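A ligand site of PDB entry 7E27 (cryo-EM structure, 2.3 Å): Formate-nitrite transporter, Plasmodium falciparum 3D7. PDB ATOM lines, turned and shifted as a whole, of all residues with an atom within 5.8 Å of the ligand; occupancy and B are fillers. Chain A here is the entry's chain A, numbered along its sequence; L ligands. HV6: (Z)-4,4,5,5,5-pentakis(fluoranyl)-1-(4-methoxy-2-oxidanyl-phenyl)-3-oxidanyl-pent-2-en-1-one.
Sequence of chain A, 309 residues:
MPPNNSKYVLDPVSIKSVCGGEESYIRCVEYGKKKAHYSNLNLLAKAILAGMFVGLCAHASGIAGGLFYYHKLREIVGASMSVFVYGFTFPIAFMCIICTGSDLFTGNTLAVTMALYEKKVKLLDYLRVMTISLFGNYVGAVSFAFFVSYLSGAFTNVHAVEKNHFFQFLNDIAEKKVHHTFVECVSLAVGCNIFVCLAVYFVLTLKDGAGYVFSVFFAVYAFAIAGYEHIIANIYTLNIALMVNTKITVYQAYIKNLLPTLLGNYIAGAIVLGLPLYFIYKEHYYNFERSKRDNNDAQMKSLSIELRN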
ATOM      1  N   TYR A  31       3.161 -21.931  20.547  1.00  0.00           N
ATOM      2  CA  TYR A  31       2.971 -20.480  20.584  1.00  0.00           C
ATOM      3  C   TYR A  31       4.047 -19.762  19.771  1.00  0.00           C
ATOM      4  O   TYR A  31       3.761 -18.732  19.148  1.00  0.00           O
ATOM      5  CB  TYR A  31       2.978 -20.013  22.043  1.00  0.00           C
ATOM      6  CG  TYR A  31       3.286 -18.552  22.249  1.00  0.00           C
ATOM      7  CD1 TYR A  31       2.317 -17.578  22.054  1.00  0.00           C
ATOM      8  CD2 TYR A  31       4.548 -18.142  22.678  1.00  0.00           C
ATOM      9  CE1 TYR A  31       2.587 -16.243  22.238  1.00  0.00           C
ATOM     10  CE2 TYR A  31       4.832 -16.805  22.867  1.00  0.00           C
ATOM     11  CZ  TYR A  31       3.851 -15.866  22.653  1.00  0.00           C
ATOM     12  OH  TYR A  31       4.135 -14.546  22.845  1.00  0.00           O
ATOM     13  N   VAL A  54       4.353  -0.867  26.565  1.00  0.00           N
ATOM     14  CA  VAL A  54       5.580  -0.767  27.364  1.00  0.00           C
ATOM     15  C   VAL A  54       5.865   0.685  27.718  1.00  0.00           C
ATOM     16  O   VAL A  54       6.172   1.010  28.875  1.00  0.00           O
ATOM     17  CB  VAL A  54       6.761  -1.417  26.609  1.00  0.00           C
ATOM     18  CG1 VAL A  54       8.085  -1.038  27.233  1.00  0.00           C
ATOM     19  CG2 VAL A  54       6.597  -2.910  26.596  1.00  0.00           C
ATOM     20  N   PHE A  90       5.449  -1.281  37.530  1.00  0.00           N
ATOM     21  CA  PHE A  90       5.710  -1.715  36.157  1.00  0.00           C
ATOM     22  C   PHE A  90       5.062  -3.014  35.619  1.00  0.00           C
ATOM     23  O   PHE A  90       4.699  -3.008  34.440  1.00  0.00           O
ATOM     24  CB  PHE A  90       7.214  -1.815  35.932  1.00  0.00           C
ATOM     25  CG  PHE A  90       7.595  -1.852  34.477  1.00  0.00           C
ATOM     26  CD1 PHE A  90       7.224  -0.825  33.628  1.00  0.00           C
ATOM     27  CD2 PHE A  90       8.298  -2.921  33.948  1.00  0.00           C
ATOM     28  CE1 PHE A  90       7.553  -0.857  32.286  1.00  0.00           C
ATOM     29  CE2 PHE A  90       8.633  -2.962  32.615  1.00  0.00           C
ATOM     30  CZ  PHE A  90       8.257  -1.926  31.780  1.00  0.00           C
ATOM     31  N   PRO A  91       4.902  -4.123  36.381  1.00  0.00           N
ATOM     32  CA  PRO A  91       4.573  -5.407  35.708  1.00  0.00           C
ATOM     33  C   PRO A  91       3.187  -5.539  35.089  1.00  0.00           C
ATOM     34  O   PRO A  91       2.860  -6.635  34.616  1.00  0.00           O
ATOM     35  CB  PRO A  91       4.750  -6.435  36.834  1.00  0.00           C
ATOM     36  CG  PRO A  91       5.633  -5.798  37.776  1.00  0.00           C
ATOM     37  CD  PRO A  91       5.194  -4.393  37.793  1.00  0.00           C
ATOM     38  N   ALA A  93       2.378  -4.233  32.375  1.00  0.00           N
ATOM     39  CA  ALA A  93       2.638  -4.233  30.929  1.00  0.00           C
ATOM     40  C   ALA A  93       2.537  -5.630  30.332  1.00  0.00           C
ATOM     41  O   ALA A  93       2.126  -5.787  29.179  1.00  0.00           O
ATOM     42  CB  ALA A  93       4.008  -3.635  30.647  1.00  0.00           C
ATOM     43  N   PHE A  94       2.917  -6.656  31.104  1.00  0.00           N
ATOM     44  CA  PHE A  94       2.788  -8.033  30.656  1.00  0.00           C
ATOM     45  C   PHE A  94       1.321  -8.400  30.407  1.00  0.00           C
ATOM     46  O   PHE A  94       1.006  -9.031  29.391  1.00  0.00           O
ATOM     47  CB  PHE A  94       3.402  -8.981  31.696  1.00  0.00           C
ATOM     48  CG  PHE A  94       3.863 -10.300  31.136  1.00  0.00           C
ATOM     49  CD1 PHE A  94       2.949 -11.311  30.851  1.00  0.00           C
ATOM     50  CD2 PHE A  94       5.200 -10.541  30.926  1.00  0.00           C
ATOM     51  CE1 PHE A  94       3.371 -12.513  30.345  1.00  0.00           C
ATOM     52  CE2 PHE A  94       5.630 -11.748  30.420  1.00  0.00           C
ATOM     53  CZ  PHE A  94       4.715 -12.726  30.128  1.00  0.00           C
ATOM     54  N   ILE A  97       0.068  -6.686  27.287  1.00  0.00           N
ATOM     55  CA  ILE A  97       0.532  -7.294  26.046  1.00  0.00           C
ATOM     56  C   ILE A  97      -0.176  -8.629  25.803  1.00  0.00           C
ATOM     57  O   ILE A  97      -0.602  -8.917  24.677  1.00  0.00           O
ATOM     58  CB  ILE A  97       2.064  -7.439  26.055  1.00  0.00           C
ATOM     59  CG1 ILE A  97       2.713  -6.061  25.952  1.00  0.00           C
ATOM     60  CG2 ILE A  97       2.566  -8.301  24.912  1.00  0.00           C
ATOM     61  CD1 ILE A  97       4.114  -6.007  26.482  1.00  0.00           C
ATOM     62  N   ILE A  98      -0.347  -9.452  26.841  1.00  0.00           N
ATOM     63  CA  ILE A  98      -0.874 -10.790  26.621  1.00  0.00           C
ATOM     64  C   ILE A  98      -2.390 -10.747  26.388  1.00  0.00           C
ATOM     65  O   ILE A  98      -2.927 -11.564  25.624  1.00  0.00           O
ATOM     66  CB  ILE A  98      -0.491 -11.748  27.777  1.00  0.00           C
ATOM     67  CG1 ILE A  98      -0.784 -13.192  27.379  1.00  0.00           C
ATOM     68  CG2 ILE A  98      -1.197 -11.432  29.092  1.00  0.00           C
ATOM     69  CD1 ILE A  98      -0.262 -14.217  28.337  1.00  0.00           C
ATOM     70  N   SER A 102      -0.694  -9.221  21.574  1.00  0.00           N
ATOM     71  CA  SER A 102       0.427  -8.607  20.895  1.00  0.00           C
ATOM     72  C   SER A 102       1.732  -9.310  21.269  1.00  0.00           C
ATOM     73  O   SER A 102       1.776 -10.146  22.176  1.00  0.00           O
ATOM     74  CB  SER A 102       0.481  -7.118  21.206  1.00  0.00           C
ATOM     75  OG  SER A 102       0.091  -6.854  22.535  1.00  0.00           O
ATOM     76  N   ASP A 103       2.809  -8.957  20.572  1.00  0.00           N
ATOM     77  CA  ASP A 103       4.079  -9.643  20.718  1.00  0.00           C
ATOM     78  C   ASP A 103       5.215  -8.657  20.971  1.00  0.00           C
ATOM     79  O   ASP A 103       5.238  -7.567  20.389  1.00  0.00           O
ATOM     80  CB  ASP A 103       4.364 -10.534  19.493  1.00  0.00           C
ATOM     81  CG  ASP A 103       4.173  -9.815  18.154  1.00  0.00           C
ATOM     82  OD1 ASP A 103       4.756  -8.740  17.906  1.00  0.00           O
ATOM     83  OD2 ASP A 103       3.407 -10.340  17.316  1.00  0.00           O
ATOM     84  N   LEU A 104       6.118  -9.025  21.866  1.00  0.00           N
ATOM     85  CA  LEU A 104       7.276  -8.208  22.183  1.00  0.00           C
ATOM     86  C   LEU A 104       8.527  -9.035  21.863  1.00  0.00           C
ATOM     87  O   LEU A 104       8.469 -10.267  21.907  1.00  0.00           O
ATOM     88  CB  LEU A 104       7.234  -7.778  23.646  1.00  0.00           C
ATOM     89  CG  LEU A 104       7.985  -6.537  24.117  1.00  0.00           C
ATOM     90  CD1 LEU A 104       7.382  -5.313  23.477  1.00  0.00           C
ATOM     91  CD2 LEU A 104       7.874  -6.407  25.606  1.00  0.00           C
ATOM     92  N   PHE A 105       9.615  -8.348  21.515  1.00  0.00           N
ATOM     93  CA  PHE A 105      10.828  -9.005  21.014  1.00  0.00           C
ATOM     94  C   PHE A 105      11.471  -9.893  22.078  1.00  0.00           C
ATOM     95  O   PHE A 105      11.976 -10.983  21.758  1.00  0.00           O
ATOM     96  CB  PHE A 105      11.804  -7.920  20.535  1.00  0.00           C
ATOM     97  CG  PHE A 105      13.129  -8.448  20.055  1.00  0.00           C
ATOM     98  CD1 PHE A 105      13.277  -8.911  18.764  1.00  0.00           C
ATOM     99  CD2 PHE A 105      14.251  -8.434  20.889  1.00  0.00           C
ATOM    100  CE1 PHE A 105      14.496  -9.384  18.315  1.00  0.00           C
ATOM    101  CE2 PHE A 105      15.467  -8.911  20.449  1.00  0.00           C
ATOM    102  CZ  PHE A 105      15.586  -9.381  19.157  1.00  0.00           C
ATOM    103  N   THR A 106      11.432  -9.444  23.336  1.00  0.00           N
ATOM    104  CA  THR A 106      12.156 -10.107  24.411  1.00  0.00           C
ATOM    105  C   THR A 106      11.599 -11.488  24.719  1.00  0.00           C
ATOM    106  O   THR A 106      12.354 -12.440  24.923  1.00  0.00           O
ATOM    107  CB  THR A 106      12.119  -9.227  25.663  1.00  0.00           C
ATOM    108  OG1 THR A 106      10.766  -8.947  26.022  1.00  0.00           O
ATOM    109  CG2 THR A 106      12.852  -7.929  25.420  1.00  0.00           C
ATOM    110  N   GLY A 107      10.273 -11.627  24.712  1.00  0.00           N
ATOM    111  CA  GLY A 107       9.681 -12.943  24.871  1.00  0.00           C
ATOM    112  C   GLY A 107       9.762 -13.776  23.607  1.00  0.00           C
ATOM    113  O   GLY A 107       9.719 -15.007  23.677  1.00  0.00           O
ATOM    114  N   ASN A 108       9.872 -13.125  22.452  1.00  0.00           N
ATOM    115  CA  ASN A 108       9.956 -13.863  21.187  1.00  0.00           C
ATOM    116  C   ASN A 108      11.300 -14.564  21.040  1.00  0.00           C
ATOM    117  O   ASN A 108      11.362 -15.627  20.412  1.00  0.00           O
ATOM    118  CB  ASN A 108       9.739 -12.926  20.009  1.00  0.00           C
ATOM    119  CG  ASN A 108       8.284 -12.615  19.767  1.00  0.00           C
ATOM    120  OD1 ASN A 108       7.420 -13.034  20.547  1.00  0.00           O
ATOM    121  ND2 ASN A 108       7.999 -11.894  18.699  1.00  0.00           N
ATOM    122  N   VAL A 196      12.350 -12.442  31.830  1.00  0.00           N
ATOM    123  CA  VAL A 196      11.261 -12.184  30.881  1.00  0.00           C
ATOM    124  C   VAL A 196      10.773 -13.490  30.245  1.00  0.00           C
ATOM    125  O   VAL A 196       9.570 -13.766  30.186  1.00  0.00           O
ATOM    126  CB  VAL A 196      11.709 -11.164  29.814  1.00  0.00           C
ATOM    127  CG1 VAL A 196      10.762 -11.147  28.633  1.00  0.00           C
ATOM    128  CG2 VAL A 196      11.805  -9.776  30.429  1.00  0.00           C
ATOM    129  N   ALA A 199       8.863 -15.515  32.694  1.00  0.00           N
ATOM    130  CA  ALA A 199       7.482 -15.050  32.859  1.00  0.00           C
ATOM    131  C   ALA A 199       6.592 -15.504  31.705  1.00  0.00           C
ATOM    132  O   ALA A 199       5.396 -15.786  31.905  1.00  0.00           O
ATOM    133  CB  ALA A 199       7.454 -13.527  32.994  1.00  0.00           C
ATOM    134  N   VAL A 200       7.153 -15.595  30.500  1.00  0.00           N
ATOM    135  CA  VAL A 200       6.441 -16.198  29.380  1.00  0.00           C
ATOM    136  C   VAL A 200       6.132 -17.675  29.653  1.00  0.00           C
ATOM    137  O   VAL A 200       5.023 -18.155  29.401  1.00  0.00           O
ATOM    138  CB  VAL A 200       7.239 -16.003  28.074  1.00  0.00           C
ATOM    139  CG1 VAL A 200       6.650 -16.797  26.923  1.00  0.00           C
ATOM    140  CG2 VAL A 200       7.311 -14.531  27.703  1.00  0.00           C
ATOM    141  N   VAL A 203       3.145 -17.796  32.190  1.00  0.00           N
ATOM    142  CA  VAL A 203       1.789 -17.675  31.639  1.00  0.00           C
ATOM    143  C   VAL A 203       1.471 -18.836  30.720  1.00  0.00           C
ATOM    144  O   VAL A 203       0.291 -19.116  30.450  1.00  0.00           O
ATOM    145  CB  VAL A 203       1.562 -16.321  30.943  1.00  0.00           C
ATOM    146  CG1 VAL A 203       1.501 -15.208  31.944  1.00  0.00           C
ATOM    147  CG2 VAL A 203       2.596 -16.060  29.877  1.00  0.00           C
ATOM    148  N   VAL A 220       8.713  -9.653  36.894  1.00  0.00           N
ATOM    149  CA  VAL A 220       9.026  -8.380  36.270  1.00  0.00           C
ATOM    150  C   VAL A 220       9.481  -7.364  37.306  1.00  0.00           C
ATOM    151  O   VAL A 220      10.435  -6.599  37.071  1.00  0.00           O
ATOM    152  CB  VAL A 220       7.837  -7.884  35.425  1.00  0.00           C
ATOM    153  CG1 VAL A 220       8.052  -6.462  34.933  1.00  0.00           C
ATOM    154  CG2 VAL A 220       7.626  -8.797  34.240  1.00  0.00           C
ATOM    155  N   PHE A 223      13.209  -8.294  38.022  1.00  0.00           N
ATOM    156  CA  PHE A 223      14.246  -7.754  37.141  1.00  0.00           C
ATOM    157  C   PHE A 223      14.284  -6.236  37.189  1.00  0.00           C
ATOM    158  O   PHE A 223      15.313  -5.623  36.892  1.00  0.00           O
ATOM    159  CB  PHE A 223      14.158  -8.306  35.689  1.00  0.00           C
ATOM    160  CG  PHE A 223      13.208  -7.575  34.733  1.00  0.00           C
ATOM    161  CD1 PHE A 223      13.567  -6.392  34.068  1.00  0.00           C
ATOM    162  CD2 PHE A 223      12.011  -8.160  34.376  1.00  0.00           C
ATOM    163  CE1 PHE A 223      12.712  -5.775  33.186  1.00  0.00           C
ATOM    164  CE2 PHE A 223      11.162  -7.553  33.480  1.00  0.00           C
ATOM    165  CZ  PHE A 223      11.508  -6.358  32.896  1.00  0.00           C
ATOM    166  N   HIS A 230      16.344  -4.065  29.984  1.00  0.00           N
ATOM    167  CA  HIS A 230      15.327  -4.487  29.026  1.00  0.00           C
ATOM    168  C   HIS A 230      15.367  -3.561  27.820  1.00  0.00           C
ATOM    169  O   HIS A 230      15.327  -2.344  27.992  1.00  0.00           O
ATOM    170  CB  HIS A 230      13.934  -4.430  29.690  1.00  0.00           C
ATOM    171  CG  HIS A 230      12.839  -5.069  28.895  1.00  0.00           C
ATOM    172  ND1 HIS A 230      12.262  -4.456  27.802  1.00  0.00           N
ATOM    173  CD2 HIS A 230      12.200  -6.239  29.051  1.00  0.00           C
ATOM    174  CE1 HIS A 230      11.315  -5.235  27.320  1.00  0.00           C
ATOM    175  NE2 HIS A 230      11.261  -6.329  28.050  1.00  0.00           N
HETATM  176  C12 HV6 L   1       8.008  -8.307  28.651  1.00  0.00           C
HETATM  177  C14 HV6 L   1       8.001  -7.492  29.949  1.00  0.00           C
HETATM  178  C01 HV6 L   1       2.342 -14.021  25.563  1.00  0.00           C
HETATM  179  C03 HV6 L   1       3.330 -11.939  25.927  1.00  0.00           C
HETATM  180  C04 HV6 L   1       4.478 -12.048  25.162  1.00  0.00           C
HETATM  181  C05 HV6 L   1       5.614 -11.357  25.529  1.00  0.00           C
HETATM  182  C06 HV6 L   1       5.604 -10.552  26.652  1.00  0.00           C
HETATM  183  C07 HV6 L   1       4.456 -10.425  27.413  1.00  0.00           C
HETATM  184  C08 HV6 L   1       3.318 -11.121  27.055  1.00  0.00           C
HETATM  185  C09 HV6 L   1       6.876  -9.801  27.014  1.00  0.00           C
HETATM  186  C11 HV6 L   1       6.927  -8.971  28.289  1.00  0.00           C
HETATM  187  C15 HV6 L   1       7.263  -6.163  29.830  1.00  0.00           C
HETATM  188  F16 HV6 L   1       7.795  -5.434  28.823  1.00  0.00           F
HETATM  189  F17 HV6 L   1       5.936  -6.361  29.616  1.00  0.00           F
HETATM  190  F18 HV6 L   1       7.405  -5.494  30.999  1.00  0.00           F
HETATM  191  F19 HV6 L   1       9.282  -7.228  30.306  1.00  0.00           F
HETATM  192  F20 HV6 L   1       7.424  -8.233  30.939  1.00  0.00           F
HETATM  193  O02 HV6 L   1       2.181 -12.632  25.556  1.00  0.00           O
HETATM  194  O10 HV6 L   1       7.820  -9.877  26.312  1.00  0.00           O
HETATM  195  O13 HV6 L   1       6.771 -11.452  24.774  1.00  0.00           O
HETATM  196  O21 HV6 L   1       9.171  -8.357  27.884  1.00  0.00           O
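NE2 of His 230 lies within hydrogen-bond range of O21 of the ligand (2.9 Å). An oxygen (O21) of the ligand is in hydrogen-bond range of the side-chain hydroxyl of Thr 106 (2.5 Å). An oxygen (O10) of the ligand sits at hydrogen-bond distance from the backbone NH (N) of Gly 107, 3.4 Å away.
OD1 of Asn 108 lies close to O of Leu 104, at 3.3 Å. The side-chain hydroxyl (OG1) of Thr 106 sits at hydrogen-bond distance from a ring nitrogen (NE2) of His 230 (3.3 Å). The backbone carbonyl oxygen (O) of Ile 97 lies within hydrogen-bond range of the side-chain hydroxyl (OG) of Ser 102, at 3.1 Å.
The backbone NH (N) of Phe 94 sits close to a fluorine (F17) of the ligand. Merely in contact with the ligand: Tyr 31 (3.3 Å), Val 54 (3.6 Å), Phe 90 (3.2 Å), Ala 93 (3.5 Å), Ile 97 (3.6 Å), Ile 98 (3.5 Å), Leu 104 (3.3 Å), Val 196 (3.3 Å), Val 220 (3.4 Å) and Phe 223 (3.5 Å). Hydrophobic or aromatic side chains that line the ligand: Tyr 31, Val 54, Phe 90, Ala 93, Phe 94, Ile 97, Ile 98, Leu 104, Val 196, Val 220, Phe 223 and His 230. Of the 22 residues printed, 14 come within 4 Å of the ligand. The nearest printed residue that does not touch the ligand is Val 200 (4.2 Å).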
